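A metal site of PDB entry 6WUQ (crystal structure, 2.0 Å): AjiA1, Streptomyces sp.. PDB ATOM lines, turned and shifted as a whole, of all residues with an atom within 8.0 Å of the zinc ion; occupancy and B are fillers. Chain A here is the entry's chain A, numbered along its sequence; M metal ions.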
ATOM      1  N   GLY A 246     -33.153  10.252  33.091  1.00  0.00           N
ATOM      2  CA  GLY A 246     -33.989   9.149  32.662  1.00  0.00           C
ATOM      3  C   GLY A 246     -33.438   8.541  31.386  1.00  0.00           C
ATOM      4  O   GLY A 246     -32.745   9.200  30.601  1.00  0.00           O
ATOM      5  N   GLN A 247     -33.742   7.261  31.181  1.00  0.00           N
ATOM      6  CA  GLN A 247     -33.207   6.536  30.040  1.00  0.00           C
ATOM      7  C   GLN A 247     -33.968   6.881  28.775  1.00  0.00           C
ATOM      8  O   GLN A 247     -35.180   7.107  28.802  1.00  0.00           O
ATOM      9  CB  GLN A 247     -33.253   5.016  30.282  1.00  0.00           C
ATOM     10  CG  GLN A 247     -31.873   4.354  30.293  1.00  0.00           C
ATOM     11  CD  GLN A 247     -31.913   2.877  30.705  1.00  0.00           C
ATOM     12  OE1 GLN A 247     -32.986   2.284  30.928  1.00  0.00           O
ATOM     13  NE2 GLN A 247     -30.718   2.281  30.821  1.00  0.00           N
ATOM     14  N   CYS A 248     -33.262   6.937  27.664  1.00  0.00           N
ATOM     15  CA  CYS A 248     -33.800   6.990  26.312  1.00  0.00           C
ATOM     16  C   CYS A 248     -33.795   5.584  25.711  1.00  0.00           C
ATOM     17  O   CYS A 248     -33.244   4.646  26.311  1.00  0.00           O
ATOM     18  CB  CYS A 248     -32.956   7.942  25.457  1.00  0.00           C
ATOM     19  SG  CYS A 248     -31.340   7.234  25.044  1.00  0.00           S
ATOM     20  N   PRO A 249     -34.395   5.374  24.533  1.00  0.00           N
ATOM     21  CA  PRO A 249     -34.377   4.026  23.936  1.00  0.00           C
ATOM     22  C   PRO A 249     -32.989   3.534  23.545  1.00  0.00           C
ATOM     23  O   PRO A 249     -32.799   2.318  23.354  1.00  0.00           O
ATOM     24  CB  PRO A 249     -35.280   4.165  22.700  1.00  0.00           C
ATOM     25  CG  PRO A 249     -36.112   5.356  22.950  1.00  0.00           C
ATOM     26  CD  PRO A 249     -35.261   6.281  23.760  1.00  0.00           C
ATOM     27  N   GLU A 250     -31.999   4.420  23.419  1.00  0.00           N
ATOM     28  CA  GLU A 250     -30.649   3.960  23.138  1.00  0.00           C
ATOM     29  C   GLU A 250     -29.960   3.401  24.368  1.00  0.00           C
ATOM     30  O   GLU A 250     -28.856   2.855  24.242  1.00  0.00           O
ATOM     31  CB  GLU A 250     -29.796   5.085  22.535  1.00  0.00           C
ATOM     32  CG  GLU A 250     -30.523   5.929  21.504  1.00  0.00           C
ATOM     33  CD  GLU A 250     -30.507   5.326  20.105  1.00  0.00           C
ATOM     34  OE1 GLU A 250     -29.749   4.361  19.859  1.00  0.00           O
ATOM     35  OE2 GLU A 250     -31.265   5.816  19.254  1.00  0.00           O
ATOM     36  N   GLY A 251     -30.576   3.497  25.548  1.00  0.00           N
ATOM     37  CA  GLY A 251     -29.993   2.965  26.754  1.00  0.00           C
ATOM     38  C   GLY A 251     -29.181   3.948  27.585  1.00  0.00           C
ATOM     39  O   GLY A 251     -28.651   3.554  28.627  1.00  0.00           O
ATOM     40  N   ARG A 252     -29.096   5.206  27.169  1.00  0.00           N
ATOM     41  CA  ARG A 252     -28.364   6.227  27.897  1.00  0.00           C
ATOM     42  C   ARG A 252     -29.286   6.988  28.831  1.00  0.00           C
ATOM     43  O   ARG A 252     -30.487   7.101  28.603  1.00  0.00           O
ATOM     44  CB  ARG A 252     -27.678   7.197  26.917  1.00  0.00           C
ATOM     45  CG  ARG A 252     -26.651   6.528  26.032  1.00  0.00           C
ATOM     46  CD  ARG A 252     -25.653   7.561  25.478  1.00  0.00           C
ATOM     47  NE  ARG A 252     -25.766   7.722  24.040  1.00  0.00           N
ATOM     48  CZ  ARG A 252     -25.121   6.954  23.168  1.00  0.00           C
ATOM     49  NH1 ARG A 252     -24.315   5.994  23.603  1.00  0.00           N
ATOM     50  NH2 ARG A 252     -25.266   7.160  21.868  1.00  0.00           N
ATOM     51  N   MET A 253     -28.727   7.506  29.919  1.00  0.00           N
ATOM     52  CA  MET A 253     -29.500   8.309  30.857  1.00  0.00           C
ATOM     53  C   MET A 253     -29.256   9.786  30.583  1.00  0.00           C
ATOM     54  O   MET A 253     -28.124  10.250  30.667  1.00  0.00           O
ATOM     55  CB  MET A 253     -29.159   7.955  32.298  1.00  0.00           C
ATOM     56  CG  MET A 253     -29.733   6.590  32.674  1.00  0.00           C
ATOM     57  SD  MET A 253     -30.168   6.513  34.408  1.00  0.00           S
ATOM     58  CE  MET A 253     -28.531   6.389  35.124  1.00  0.00           C
ATOM     59  N   HIS A 254     -30.323  10.516  30.266  1.00  0.00           N
ATOM     60  CA  HIS A 254     -30.244  11.929  29.946  1.00  0.00           C
ATOM     61  C   HIS A 254     -30.620  12.763  31.159  1.00  0.00           C
ATOM     62  O   HIS A 254     -31.716  12.599  31.716  1.00  0.00           O
ATOM     63  CB  HIS A 254     -31.171  12.271  28.768  1.00  0.00           C
ATOM     64  CG  HIS A 254     -30.617  11.883  27.426  1.00  0.00           C
ATOM     65  ND1 HIS A 254     -29.921  12.755  26.621  1.00  0.00           N
ATOM     66  CD2 HIS A 254     -30.664  10.708  26.743  1.00  0.00           C
ATOM     67  CE1 HIS A 254     -29.575  12.144  25.497  1.00  0.00           C
ATOM     68  NE2 HIS A 254     -30.004  10.904  25.558  1.00  0.00           N
ATOM     69  N   ASP A 306     -21.785  14.423  24.444  1.00  0.00           N
ATOM     70  CA  ASP A 306     -21.869  13.909  23.082  1.00  0.00           C
ATOM     71  C   ASP A 306     -23.323  13.645  22.703  1.00  0.00           C
ATOM     72  O   ASP A 306     -24.035  12.971  23.442  1.00  0.00           O
ATOM     73  CB  ASP A 306     -21.046  12.637  22.923  1.00  0.00           C
ATOM     74  CG  ASP A 306     -19.575  12.845  23.223  1.00  0.00           C
ATOM     75  OD1 ASP A 306     -19.171  14.020  23.418  1.00  0.00           O
ATOM     76  OD2 ASP A 306     -18.826  11.849  23.265  1.00  0.00           O
ATOM     77  N   PRO A 307     -23.794  14.174  21.569  1.00  0.00           N
ATOM     78  CA  PRO A 307     -25.199  14.018  21.206  1.00  0.00           C
ATOM     79  C   PRO A 307     -25.617  12.552  21.136  1.00  0.00           C
ATOM     80  O   PRO A 307     -24.798  11.661  20.894  1.00  0.00           O
ATOM     81  CB  PRO A 307     -25.286  14.692  19.832  1.00  0.00           C
ATOM     82  CG  PRO A 307     -24.105  15.621  19.781  1.00  0.00           C
ATOM     83  CD  PRO A 307     -23.029  14.939  20.567  1.00  0.00           C
ATOM     84  N   CYS A 308     -26.913  12.320  21.339  1.00  0.00           N
ATOM     85  CA  CYS A 308     -27.468  10.977  21.289  1.00  0.00           C
ATOM     86  C   CYS A 308     -28.526  10.859  20.195  1.00  0.00           C
ATOM     87  O   CYS A 308     -29.383  11.745  20.063  1.00  0.00           O
ATOM     88  CB  CYS A 308     -28.101  10.617  22.646  1.00  0.00           C
ATOM     89  SG  CYS A 308     -28.646   8.902  22.723  1.00  0.00           S
ATOM     90  N   PRO A 309     -28.524   9.765  19.423  1.00  0.00           N
ATOM     91  CA  PRO A 309     -29.474   9.665  18.306  1.00  0.00           C
ATOM     92  C   PRO A 309     -30.928   9.537  18.708  1.00  0.00           C
ATOM     93  O   PRO A 309     -31.795   9.441  17.827  1.00  0.00           O
ATOM     94  CB  PRO A 309     -28.994   8.405  17.547  1.00  0.00           C
ATOM     95  CG  PRO A 309     -28.168   7.639  18.531  1.00  0.00           C
ATOM     96  CD  PRO A 309     -27.535   8.673  19.419  1.00  0.00           C
ATOM     97  N   CYS A 310     -31.251   9.559  20.013  1.00  0.00           N
ATOM     98  CA  CYS A 310     -32.657   9.434  20.411  1.00  0.00           C
ATOM     99  C   CYS A 310     -33.452  10.702  20.129  1.00  0.00           C
ATOM    100  O   CYS A 310     -34.684  10.638  20.063  1.00  0.00           O
ATOM    101  CB  CYS A 310     -32.771   9.078  21.907  1.00  0.00           C
ATOM    102  SG  CYS A 310     -32.167  10.421  23.014  1.00  0.00           S
ATOM    103  N   GLY A 311     -32.787  11.848  19.969  1.00  0.00           N
ATOM    104  CA  GLY A 311     -33.446  13.113  19.758  1.00  0.00           C
ATOM    105  C   GLY A 311     -33.483  14.034  20.966  1.00  0.00           C
ATOM    106  O   GLY A 311     -33.712  15.236  20.792  1.00  0.00           O
ATOM    107  N   TRP A 312     -33.261  13.507  22.166  1.00  0.00           N
ATOM    108  CA  TRP A 312     -33.256  14.332  23.376  1.00  0.00           C
ATOM    109  C   TRP A 312     -31.980  15.164  23.407  1.00  0.00           C
ATOM    110  O   TRP A 312     -30.889  14.617  23.591  1.00  0.00           O
ATOM    111  CB  TRP A 312     -33.393  13.449  24.610  1.00  0.00           C
ATOM    112  CG  TRP A 312     -34.810  13.281  25.142  1.00  0.00           C
ATOM    113  CD1 TRP A 312     -35.884  14.102  24.914  1.00  0.00           C
ATOM    114  CD2 TRP A 312     -35.295  12.223  25.997  1.00  0.00           C
ATOM    115  NE1 TRP A 312     -37.000  13.633  25.567  1.00  0.00           N
ATOM    116  CE2 TRP A 312     -36.673  12.481  26.238  1.00  0.00           C
ATOM    117  CE3 TRP A 312     -34.702  11.098  26.584  1.00  0.00           C
ATOM    118  CZ2 TRP A 312     -37.454  11.639  27.030  1.00  0.00           C
ATOM    119  CZ3 TRP A 312     -35.492  10.259  27.366  1.00  0.00           C
ATOM    120  CH2 TRP A 312     -36.844  10.534  27.579  1.00  0.00           C
ATOM    121  N   LEU A 313     -32.097  16.480  23.234  1.00  0.00           N
ATOM    122  CA  LEU A 313     -30.933  17.367  23.196  1.00  0.00           C
ATOM    123  C   LEU A 313     -30.499  17.686  24.629  1.00  0.00           C
ATOM    124  O   LEU A 313     -30.620  18.811  25.119  1.00  0.00           O
ATOM    125  CB  LEU A 313     -31.245  18.634  22.419  1.00  0.00           C
ATOM    126  CG  LEU A 313     -31.659  18.395  20.972  1.00  0.00           C
ATOM    127  CD1 LEU A 313     -31.759  19.730  20.239  1.00  0.00           C
ATOM    128  CD2 LEU A 313     -30.654  17.474  20.298  1.00  0.00           C
ATOM    129  N   LEU A 314     -30.019  16.649  25.302  1.00  0.00           N
ATOM    130  CA  LEU A 314     -29.618  16.745  26.682  1.00  0.00           C
ATOM    131  C   LEU A 314     -28.372  15.909  26.956  1.00  0.00           C
ATOM    132  O   LEU A 314     -28.241  14.803  26.404  1.00  0.00           O
ATOM    133  CB  LEU A 314     -30.751  16.300  27.617  1.00  0.00           C
ATOM    134  CG  LEU A 314     -32.042  17.153  27.619  1.00  0.00           C
ATOM    135  CD1 LEU A 314     -33.255  16.378  28.127  1.00  0.00           C
ATOM    136  CD2 LEU A 314     -31.815  18.461  28.441  1.00  0.00           C
ATOM    137  N   PRO A 315     -27.456  16.387  27.804  1.00  0.00           N
ATOM    138  CA  PRO A 315     -26.267  15.595  28.122  1.00  0.00           C
ATOM    139  C   PRO A 315     -26.632  14.302  28.815  1.00  0.00           C
ATOM    140  O   PRO A 315     -27.747  14.135  29.330  1.00  0.00           O
ATOM    141  CB  PRO A 315     -25.457  16.528  29.046  1.00  0.00           C
ATOM    142  CG  PRO A 315     -26.465  17.486  29.599  1.00  0.00           C
ATOM    143  CD  PRO A 315     -27.493  17.664  28.533  1.00  0.00           C
ATOM    144  N   THR A 316     -25.723  13.344  28.774  1.00  0.00           N
ATOM    145  CA  THR A 316     -25.997  12.041  29.365  1.00  0.00           C
ATOM    146  C   THR A 316     -25.065  11.812  30.540  1.00  0.00           C
ATOM    147  O   THR A 316     -24.021  12.463  30.677  1.00  0.00           O
ATOM    148  CB  THR A 316     -25.865  10.914  28.333  1.00  0.00           C
ATOM    149  OG1 THR A 316     -24.519  10.882  27.838  1.00  0.00           O
ATOM    150  CG2 THR A 316     -26.813  11.139  27.171  1.00  0.00           C
HETATM  151 ZN    ZN M   1     -30.518   9.227  24.104  1.00  0.00          ZN
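ND1 of His 254 is in hydrogen-bond range of O of Leu 314 (2.7 Å).
The backbone NH (N) of His 254 sits at hydrogen-bond distance from the backbone carbonyl oxygen (O) of Gly 246.
N of Trp 312 lies close to SG of Cys 310, at 3.4 Å.
SG of Cys 308 sits close to NE of Arg 252 (3.4 Å).
The side-chain sulfur (SG) of Cys 248 lies close to the backbone NH (N) of Glu 250, 3.3 Å away.
The side-chain sulfur of Cys 248 lies close to the backbone carbonyl oxygen of Arg 252.
The zinc ion is bound by a ring nitrogen (NE2) of His 254 (2.3 Å), the side-chain sulfur (SG) of Cys 310 (2.3 Å), the side-chain sulfur (SG) of Cys 308 (2.3 Å) and the side-chain sulfur (SG) of Cys 248 (2.4 Å).
The zinc ion has four donor atoms within binding distance.
Within 4 Å of the zinc ion: Cys 248, His 254, Cys 308 and Cys 310.
The nearest printed residue that does not touch the zinc ion is Glu 250 (4.2 Å).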
